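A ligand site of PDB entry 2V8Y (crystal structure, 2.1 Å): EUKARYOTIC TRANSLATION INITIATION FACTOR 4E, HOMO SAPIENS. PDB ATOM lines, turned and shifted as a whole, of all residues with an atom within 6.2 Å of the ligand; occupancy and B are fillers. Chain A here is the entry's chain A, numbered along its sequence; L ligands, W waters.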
ATOM      1  N   PHE A  48       4.875 -11.539   3.657  1.00  0.00           N
ATOM      2  CA  PHE A  48       5.366 -11.514   2.266  1.00  0.00           C
ATOM      3  C   PHE A  48       6.637 -10.671   2.169  1.00  0.00           C
ATOM      4  O   PHE A  48       6.668  -9.533   2.594  1.00  0.00           O
ATOM      5  CB  PHE A  48       4.317 -10.898   1.329  1.00  0.00           C
ATOM      6  CG  PHE A  48       4.735 -10.868  -0.122  1.00  0.00           C
ATOM      7  CD1 PHE A  48       4.370 -11.894  -0.979  1.00  0.00           C
ATOM      8  CD2 PHE A  48       5.477  -9.791  -0.637  1.00  0.00           C
ATOM      9  CE1 PHE A  48       4.758 -11.880  -2.332  1.00  0.00           C
ATOM     10  CE2 PHE A  48       5.877  -9.781  -1.972  1.00  0.00           C
ATOM     11  CZ  PHE A  48       5.507 -10.828  -2.835  1.00  0.00           C
ATOM     12  N   TRP A  56       4.982 -15.448  -6.936  1.00  0.00           N
ATOM     13  CA  TRP A  56       4.364 -14.598  -5.914  1.00  0.00           C
ATOM     14  C   TRP A  56       3.969 -15.458  -4.675  1.00  0.00           C
ATOM     15  O   TRP A  56       4.353 -15.132  -3.543  1.00  0.00           O
ATOM     16  CB  TRP A  56       3.172 -13.813  -6.492  1.00  0.00           C
ATOM     17  CG  TRP A  56       2.549 -12.972  -5.468  1.00  0.00           C
ATOM     18  CD1 TRP A  56       2.932 -11.723  -5.096  1.00  0.00           C
ATOM     19  CD2 TRP A  56       1.490 -13.355  -4.594  1.00  0.00           C
ATOM     20  NE1 TRP A  56       2.145 -11.283  -4.067  1.00  0.00           N
ATOM     21  CE2 TRP A  56       1.260 -12.270  -3.723  1.00  0.00           C
ATOM     22  CE3 TRP A  56       0.703 -14.510  -4.455  1.00  0.00           C
ATOM     23  CZ2 TRP A  56       0.265 -12.294  -2.721  1.00  0.00           C
ATOM     24  CZ3 TRP A  56      -0.271 -14.535  -3.467  1.00  0.00           C
ATOM     25  CH2 TRP A  56      -0.484 -13.426  -2.609  1.00  0.00           C
ATOM     26  N   GLN A  57       3.255 -16.559  -4.920  1.00  0.00           N
ATOM     27  CA  GLN A  57       2.826 -17.495  -3.855  1.00  0.00           C
ATOM     28  C   GLN A  57       3.940 -17.978  -2.938  1.00  0.00           C
ATOM     29  O   GLN A  57       3.734 -18.066  -1.705  1.00  0.00           O
ATOM     30  CB  GLN A  57       2.150 -18.725  -4.465  1.00  0.00           C
ATOM     31  CG  GLN A  57       0.693 -18.609  -4.669  1.00  0.00           C
ATOM     32  CD  GLN A  57       0.070 -19.961  -5.021  1.00  0.00           C
ATOM     33  OE1 GLN A  57      -0.539 -20.122  -6.087  1.00  0.00           O
ATOM     34  NE2 GLN A  57       0.200 -20.930  -4.136  1.00  0.00           N
ATOM     35  N   ASP A  90       4.651  -7.369   3.033  1.00  0.00           N
ATOM     36  CA  ASP A  90       3.269  -7.327   3.500  1.00  0.00           C
ATOM     37  C   ASP A  90       3.102  -8.081   4.841  1.00  0.00           C
ATOM     38  O   ASP A  90       3.773  -9.112   5.057  1.00  0.00           O
ATOM     39  CB  ASP A  90       2.275  -8.010   2.556  1.00  0.00           C
ATOM     40  CG  ASP A  90       2.383  -7.601   1.108  1.00  0.00           C
ATOM     41  OD1 ASP A  90       2.952  -6.538   0.762  1.00  0.00           O
ATOM     42  OD2 ASP A  90       1.859  -8.374   0.291  1.00  0.00           O
ATOM     43  N   PRO A 100      -4.312 -15.986   1.926  1.00  0.00           N
ATOM     44  CA  PRO A 100      -4.300 -14.572   1.640  1.00  0.00           C
ATOM     45  C   PRO A 100      -3.914 -14.257   0.183  1.00  0.00           C
ATOM     46  O   PRO A 100      -2.984 -13.483  -0.070  1.00  0.00           O
ATOM     47  CB  PRO A 100      -3.291 -14.021   2.653  1.00  0.00           C
ATOM     48  CG  PRO A 100      -2.355 -15.089   2.821  1.00  0.00           C
ATOM     49  CD  PRO A 100      -3.121 -16.367   2.724  1.00  0.00           C
ATOM     50  N   MET A 101      -4.676 -14.839  -0.748  1.00  0.00           N
ATOM     51  CA  MET A 101      -4.473 -14.633  -2.180  1.00  0.00           C
ATOM     52  C   MET A 101      -5.843 -14.679  -2.888  1.00  0.00           C
ATOM     53  O   MET A 101      -6.779 -15.336  -2.389  1.00  0.00           O
ATOM     54  CB  MET A 101      -3.501 -15.709  -2.717  1.00  0.00           C
ATOM     55  CG  MET A 101      -3.988 -17.167  -2.556  1.00  0.00           C
ATOM     56  SD  MET A 101      -2.750 -18.426  -2.980  1.00  0.00           S
ATOM     57  CE  MET A 101      -1.594 -18.338  -1.641  1.00  0.00           C
ATOM     58  N   TRP A 102      -5.969 -13.985  -4.017  1.00  0.00           N
ATOM     59  CA  TRP A 102      -7.245 -13.919  -4.723  1.00  0.00           C
ATOM     60  C   TRP A 102      -7.733 -15.282  -5.300  1.00  0.00           C
ATOM     61  O   TRP A 102      -8.926 -15.447  -5.530  1.00  0.00           O
ATOM     62  CB  TRP A 102      -7.275 -12.778  -5.778  1.00  0.00           C
ATOM     63  CG  TRP A 102      -6.263 -12.885  -6.932  1.00  0.00           C
ATOM     64  CD1 TRP A 102      -5.973 -13.983  -7.688  1.00  0.00           C
ATOM     65  CD2 TRP A 102      -5.420 -11.824  -7.441  1.00  0.00           C
ATOM     66  NE1 TRP A 102      -5.014 -13.694  -8.621  1.00  0.00           N
ATOM     67  CE2 TRP A 102      -4.656 -12.368  -8.500  1.00  0.00           C
ATOM     68  CE3 TRP A 102      -5.241 -10.468  -7.112  1.00  0.00           C
ATOM     69  CZ2 TRP A 102      -3.715 -11.602  -9.236  1.00  0.00           C
ATOM     70  CZ3 TRP A 102      -4.309  -9.708  -7.839  1.00  0.00           C
ATOM     71  CH2 TRP A 102      -3.558 -10.279  -8.893  1.00  0.00           C
ATOM     72  N   GLU A 103      -6.820 -16.235  -5.503  1.00  0.00           N
ATOM     73  CA  GLU A 103      -7.145 -17.591  -6.017  1.00  0.00           C
ATOM     74  C   GLU A 103      -7.999 -18.420  -5.041  1.00  0.00           C
ATOM     75  O   GLU A 103      -8.554 -19.440  -5.428  1.00  0.00           O
ATOM     76  CB  GLU A 103      -5.869 -18.420  -6.224  1.00  0.00           C
ATOM     77  CG  GLU A 103      -4.908 -17.964  -7.312  1.00  0.00           C
ATOM     78  CD  GLU A 103      -3.825 -17.029  -6.808  1.00  0.00           C
ATOM     79  OE1 GLU A 103      -4.070 -16.143  -5.962  1.00  0.00           O
ATOM     80  OE2 GLU A 103      -2.691 -17.167  -7.297  1.00  0.00           O
ATOM     81  N   ARG A 112     -12.046  -5.954  -1.883  1.00  0.00           N
ATOM     82  CA  ARG A 112     -11.449  -5.355  -0.696  1.00  0.00           C
ATOM     83  C   ARG A 112     -11.812  -3.875  -0.576  1.00  0.00           C
ATOM     84  O   ARG A 112     -11.947  -3.182  -1.591  1.00  0.00           O
ATOM     85  CB  ARG A 112      -9.948  -5.461  -0.815  1.00  0.00           C
ATOM     86  CG  ARG A 112      -9.350  -4.319  -1.598  1.00  0.00           C
ATOM     87  CD  ARG A 112      -8.422  -4.724  -2.691  1.00  0.00           C
ATOM     88  NE  ARG A 112      -7.035  -4.718  -2.275  1.00  0.00           N
ATOM     89  CZ  ARG A 112      -6.011  -4.251  -2.999  1.00  0.00           C
ATOM     90  NH1 ARG A 112      -6.186  -3.685  -4.172  1.00  0.00           N
ATOM     91  NH2 ARG A 112      -4.795  -4.329  -2.503  1.00  0.00           N
ATOM     92  N   VAL A 153      -4.903  -6.969   4.722  1.00  0.00           N
ATOM     93  CA  VAL A 153      -3.473  -6.882   4.380  1.00  0.00           C
ATOM     94  C   VAL A 153      -2.922  -5.443   4.385  1.00  0.00           C
ATOM     95  O   VAL A 153      -3.583  -4.505   3.952  1.00  0.00           O
ATOM     96  CB  VAL A 153      -3.003  -7.817   3.121  1.00  0.00           C
ATOM     97  CG1 VAL A 153      -4.159  -8.651   2.439  1.00  0.00           C
ATOM     98  CG2 VAL A 153      -2.031  -7.148   2.133  1.00  0.00           C
ATOM     99  N   ASN A 155       0.270  -3.440   2.871  1.00  0.00           N
ATOM    100  CA  ASN A 155       1.368  -3.383   1.904  1.00  0.00           C
ATOM    101  C   ASN A 155       2.279  -2.220   2.312  1.00  0.00           C
ATOM    102  O   ASN A 155       1.839  -1.079   2.396  1.00  0.00           O
ATOM    103  CB  ASN A 155       0.818  -3.081   0.503  1.00  0.00           C
ATOM    104  CG  ASN A 155      -0.250  -4.058   0.068  1.00  0.00           C
ATOM    105  OD1 ASN A 155      -1.354  -3.659  -0.240  1.00  0.00           O
ATOM    106  ND2 ASN A 155       0.093  -5.319  -0.017  1.00  0.00           N
ATOM    107  N   ARG A 157       5.128   0.026   0.988  1.00  0.00           N
ATOM    108  CA  ARG A 157       5.685   0.354  -0.335  1.00  0.00           C
ATOM    109  C   ARG A 157       6.288   1.764  -0.353  1.00  0.00           C
ATOM    110  O   ARG A 157       5.667   2.695   0.147  1.00  0.00           O
ATOM    111  CB  ARG A 157       4.586   0.289  -1.411  1.00  0.00           C
ATOM    112  CG  ARG A 157       3.860  -1.049  -1.549  1.00  0.00           C
ATOM    113  CD  ARG A 157       4.763  -2.088  -2.132  1.00  0.00           C
ATOM    114  NE  ARG A 157       4.052  -3.349  -2.385  1.00  0.00           N
ATOM    115  CZ  ARG A 157       3.912  -4.354  -1.508  1.00  0.00           C
ATOM    116  NH1 ARG A 157       4.394  -4.266  -0.287  1.00  0.00           N
ATOM    117  NH2 ARG A 157       3.264  -5.450  -1.876  1.00  0.00           N
ATOM    118  N   LYS A 162      -0.481   0.745   1.724  1.00  0.00           N
ATOM    119  CA  LYS A 162      -1.900   0.447   1.590  1.00  0.00           C
ATOM    120  C   LYS A 162      -2.314  -0.516   2.754  1.00  0.00           C
ATOM    121  O   LYS A 162      -1.487  -1.332   3.196  1.00  0.00           O
ATOM    122  CB  LYS A 162      -2.180  -0.198   0.243  1.00  0.00           C
ATOM    123  CG  LYS A 162      -2.072   0.747  -0.999  1.00  0.00           C
ATOM    124  CD  LYS A 162      -2.074  -0.040  -2.302  1.00  0.00           C
ATOM    125  CE  LYS A 162      -0.831  -0.871  -2.477  1.00  0.00           C
ATOM    126  NZ  LYS A 162      -0.664  -1.355  -3.898  1.00  0.00           N
ATOM    127  N   TRP A 166     -10.485  -7.643   3.114  1.00  0.00           N
ATOM    128  CA  TRP A 166     -11.000  -8.450   2.021  1.00  0.00           C
ATOM    129  C   TRP A 166     -12.286  -9.074   2.483  1.00  0.00           C
ATOM    130  O   TRP A 166     -12.408  -9.495   3.648  1.00  0.00           O
ATOM    131  CB  TRP A 166     -10.014  -9.561   1.679  1.00  0.00           C
ATOM    132  CG  TRP A 166      -8.698  -9.145   1.054  1.00  0.00           C
ATOM    133  CD1 TRP A 166      -8.058  -7.946   1.180  1.00  0.00           C
ATOM    134  CD2 TRP A 166      -7.831  -9.979   0.282  1.00  0.00           C
ATOM    135  NE1 TRP A 166      -6.858  -7.964   0.501  1.00  0.00           N
ATOM    136  CE2 TRP A 166      -6.696  -9.206  -0.062  1.00  0.00           C
ATOM    137  CE3 TRP A 166      -7.894 -11.318  -0.162  1.00  0.00           C
ATOM    138  CZ2 TRP A 166      -5.648  -9.736  -0.828  1.00  0.00           C
ATOM    139  CZ3 TRP A 166      -6.865 -11.826  -0.923  1.00  0.00           C
ATOM    140  CH2 TRP A 166      -5.754 -11.041  -1.260  1.00  0.00           C
ATOM    141  N   GLN A 198     -12.976  -2.550  -4.348  1.00  0.00           N
ATOM    142  CA  GLN A 198     -12.726  -3.104  -5.667  1.00  0.00           C
ATOM    143  C   GLN A 198     -12.821  -4.588  -5.593  1.00  0.00           C
ATOM    144  O   GLN A 198     -12.276  -5.217  -4.677  1.00  0.00           O
ATOM    145  CB  GLN A 198     -11.326  -2.735  -6.178  1.00  0.00           C
ATOM    146  CG  GLN A 198     -11.104  -1.241  -6.289  1.00  0.00           C
ATOM    147  CD  GLN A 198     -10.223  -0.752  -5.208  1.00  0.00           C
ATOM    148  OE1 GLN A 198      -9.243  -1.420  -4.856  1.00  0.00           O
ATOM    149  NE2 GLN A 198     -10.546   0.424  -4.650  1.00  0.00           N
ATOM    150  N   SER A 199     -13.505  -5.161  -6.585  1.00  0.00           N
ATOM    151  CA  SER A 199     -13.569  -6.591  -6.726  1.00  0.00           C
ATOM    152  C   SER A 199     -12.199  -7.118  -7.168  1.00  0.00           C
ATOM    153  O   SER A 199     -11.495  -6.469  -7.959  1.00  0.00           O
ATOM    154  CB  SER A 199     -14.682  -6.941  -7.724  1.00  0.00           C
ATOM    155  OG  SER A 199     -14.118  -7.387  -8.937  1.00  0.00           O
ATOM    156  N   HIS A 200     -11.791  -8.263  -6.623  1.00  0.00           N
ATOM    157  CA  HIS A 200     -10.496  -8.908  -6.961  1.00  0.00           C
ATOM    158  C   HIS A 200     -10.416  -9.335  -8.444  1.00  0.00           C
ATOM    159  O   HIS A 200      -9.304  -9.393  -9.009  1.00  0.00           O
ATOM    160  CB  HIS A 200     -10.195 -10.142  -6.083  1.00  0.00           C
ATOM    161  CG  HIS A 200     -10.051  -9.862  -4.614  1.00  0.00           C
ATOM    162  ND1 HIS A 200      -9.351  -8.785  -4.122  1.00  0.00           N
ATOM    163  CD2 HIS A 200     -10.500 -10.550  -3.536  1.00  0.00           C
ATOM    164  CE1 HIS A 200      -9.388  -8.808  -2.798  1.00  0.00           C
ATOM    165  NE2 HIS A 200     -10.067  -9.879  -2.419  1.00  0.00           N
ATOM    166  N   THR A 203      -9.296  -6.172 -10.099  1.00  0.00           N
ATOM    167  CA  THR A 203      -7.871  -6.026  -9.754  1.00  0.00           C
ATOM    168  C   THR A 203      -6.921  -7.028 -10.469  1.00  0.00           C
ATOM    169  O   THR A 203      -5.859  -6.644 -10.945  1.00  0.00           O
ATOM    170  CB  THR A 203      -7.660  -6.061  -8.216  1.00  0.00           C
ATOM    171  OG1 THR A 203      -8.551  -5.113  -7.592  1.00  0.00           O
ATOM    172  CG2 THR A 203      -6.213  -5.722  -7.863  1.00  0.00           C
ATOM    173  N   ALA A 204      -7.302  -8.301 -10.539  1.00  0.00           N
ATOM    174  CA  ALA A 204      -6.498  -9.299 -11.255  1.00  0.00           C
ATOM    175  C   ALA A 204      -6.550  -9.160 -12.780  1.00  0.00           C
ATOM    176  O   ALA A 204      -5.936  -9.952 -13.499  1.00  0.00           O
ATOM    177  CB  ALA A 204      -6.867 -10.730 -10.827  1.00  0.00           C
HETATM  178  C1  LIG L   1      -3.171  -7.754  -4.505  1.00  0.00           C
HETATM  179  C2  LIG L   1      -4.270  -6.948  -4.779  1.00  0.00           C
HETATM  180  C3  LIG L   1      -5.554  -7.458  -4.605  1.00  0.00           C
HETATM  181  F1  LIG L   1      -6.614  -6.692  -4.867  1.00  0.00           F
HETATM  182  C4  LIG L   1      -5.768  -8.765  -4.186  1.00  0.00           C
HETATM  183  C5  LIG L   1      -4.694  -9.582  -3.920  1.00  0.00           C
HETATM  184  C6  LIG L   1      -3.413  -9.057  -4.078  1.00  0.00           C
HETATM  185  C7  LIG L   1      -2.272  -9.937  -3.780  1.00  0.00           C
HETATM  186  N1  LIG L   1      -1.571 -10.414  -4.975  1.00  0.00           N
HETATM  187  C8  LIG L   1      -0.573  -9.754  -5.551  1.00  0.00           C
HETATM  188  C9  LIG L   1      -1.754 -11.600  -5.546  1.00  0.00           C
HETATM  189  C10 LIG L   1      -2.637 -12.675  -5.343  1.00  0.00           C
HETATM  190  O1  LIG L   1      -3.493 -12.718  -4.456  1.00  0.00           O
HETATM  191  N2  LIG L   1      -2.517 -13.751  -6.210  1.00  0.00           N
HETATM  192  C11 LIG L   1      -1.564 -13.752  -7.222  1.00  0.00           C
HETATM  193  N3  LIG L   1      -1.493 -14.817  -8.023  1.00  0.00           N
HETATM  194  N4  LIG L   1      -0.736 -12.723  -7.387  1.00  0.00           N
HETATM  195  C12 LIG L   1      -0.831 -11.646  -6.579  1.00  0.00           C
HETATM  196  N5  LIG L   1      -0.119 -10.520  -6.555  1.00  0.00           N
HETATM  197  C13 LIG L   1       0.980 -10.185  -7.544  1.00  0.00           C
HETATM  198  O2  LIG L   1       1.718  -9.046  -7.114  1.00  0.00           O
HETATM  199  C14 LIG L   1       0.339  -9.795  -8.881  1.00  0.00           C
HETATM  200  O3  LIG L   1       1.248 -10.031  -9.953  1.00  0.00           O
HETATM  201  C15 LIG L   1       0.147  -8.299  -8.686  1.00  0.00           C
HETATM  202  O4  LIG L   1      -0.102  -7.632  -9.955  1.00  0.00           O
HETATM  203  C16 LIG L   1       1.491  -7.948  -8.059  1.00  0.00           C
HETATM  204  C17 LIG L   1       1.556  -6.697  -7.136  1.00  0.00           C
HETATM  205  O5  LIG L   1       0.489  -6.705  -6.186  1.00  0.00           O
HETATM  206  P1  LIG L   1       0.601  -5.905  -4.731  1.00  0.00           P
HETATM  207  O6  LIG L   1      -0.435  -4.685  -4.816  1.00  0.00           O
HETATM  208  O7  LIG L   1       0.005  -6.965  -3.698  1.00  0.00           O
HETATM  209  O8  LIG L   1       1.984  -5.436  -4.469  1.00  0.00           O
HETATM  210  O   HOH W   1      -2.918  -3.779  -6.222  1.00  0.00           O
HETATM  211  O   HOH W   2       4.046  -7.624  -4.317  1.00  0.00           O
HETATM  212  O   HOH W   3      -2.121  -8.756 -12.137  1.00  0.00           O
HETATM  213  O   HOH W   4       3.796  -4.016  -5.862  1.00  0.00           O
HETATM  214  O   HOH W   5      -2.149  -4.171  -2.873  1.00  0.00           O
HETATM  215  O   HOH W   6       1.219 -13.774  -9.726  1.00  0.00           O
HETATM  216  O   HOH W   7      -9.355  -6.263  -5.186  1.00  0.00           O
HETATM  217  O   HOH W   8       1.275  -2.790  -4.241  1.00  0.00           O
HETATM  218  O   HOH W   9       2.169  -8.460  -2.382  1.00  0.00           O
HETATM  219  O   HOH W  10      -2.587  -6.659  -1.597  1.00  0.00           O
HETATM  220  O   HOH W  11      -0.928  -9.696  -0.845  1.00  0.00           O
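Water W8 lies within hydrogen-bond range of NZ of Lys 162 (2.4 Å), O6 of the ligand (2.6 Å) and NE of Arg 157 (3.4 Å).
Water W5 lies within hydrogen-bond range of O6 of the ligand (2.6 Å), NH2 of Arg 112 (2.7 Å), OD1 of Asn 155 (2.8 Å) and NZ of Lys 162 (3.3 Å).
Water W7 lies within hydrogen-bond range of a ring nitrogen (ND1) of His 200 (2.7 Å), the side-chain hydroxyl (OG1) of Thr 203 (2.8 Å) and the backbone carbonyl oxygen (O) of Gln 198 (3.1 Å).
Water W9 lies within hydrogen-bond range of the side-chain carboxylate (OD2) of Asp 90, an oxygen (O7) of the ligand, the guanidinium group (NH2) of Arg 157 and the indole nitrogen (NE1) of Trp 56.
Water W2 lies within hydrogen-bond range of O8 of the ligand and NH2 of Arg 157.
Water W10 lies within hydrogen-bond range of the guanidinium group (NH2) of Arg 112 (3.3 Å), an oxygen (O7) of the ligand (3.4 Å) and the side-chain amide nitrogen (ND2) of Asn 155 (3.4 Å).
NE1 of Trp 56 lies close to N5 of the ligand (3.4 Å).
NH1 of Arg 112 lies close to F1 of the ligand, 3.1 Å away.
Met 101 touches the ligand.
Trp 166 touches the ligand (CH2 to C5, 3.2 Å).
ND1 of His 200 touches F1 of the ligand (3.5 Å).
Thr 203 touches the ligand.
Hydrophobic or aromatic side chains that line the ligand: Trp 56, Met 101, Trp 102, Trp 166 and His 200.
Ten residues have an atom within 4 Å of the ligand: Trp 56, Met 101, Trp 102, Glu 103, Arg 112, Arg 157, Lys 162, Trp 166, His 200 and Thr 203.
The nearest printed residue that does not touch the ligand is Asn 155 (4.03 Å).
OE2 of Glu 103 is in hydrogen-bond range of N3 of the ligand, at 2.7 Å.
N of Trp 102 lies within hydrogen-bond range of O1 of the ligand.
An oxygen (O8) of the ligand lies within salt-bridge range of the guanidinium group (NH2) of Arg 157, 2.9 Å away.
The side-chain amino group of Lys 162 is in salt-bridge range of an oxygen (O6) of the ligand, at 3.5 Å.
OD1 of Asp 90 lies within salt-bridge range of NH2 of Arg 157.
The backbone carbonyl oxygen (O) of Gln 198 lies within hydrogen-bond range of the backbone NH (N) of Arg 112 (2.9 Å).
O of Ser 199 sits at hydrogen-bond distance from OG1 of Thr 203, 3.3 Å away.
The backbone carbonyl oxygen (O) of Lys 162 is in hydrogen-bond range of the backbone NH (N) of Asn 155 (2.8 Å).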
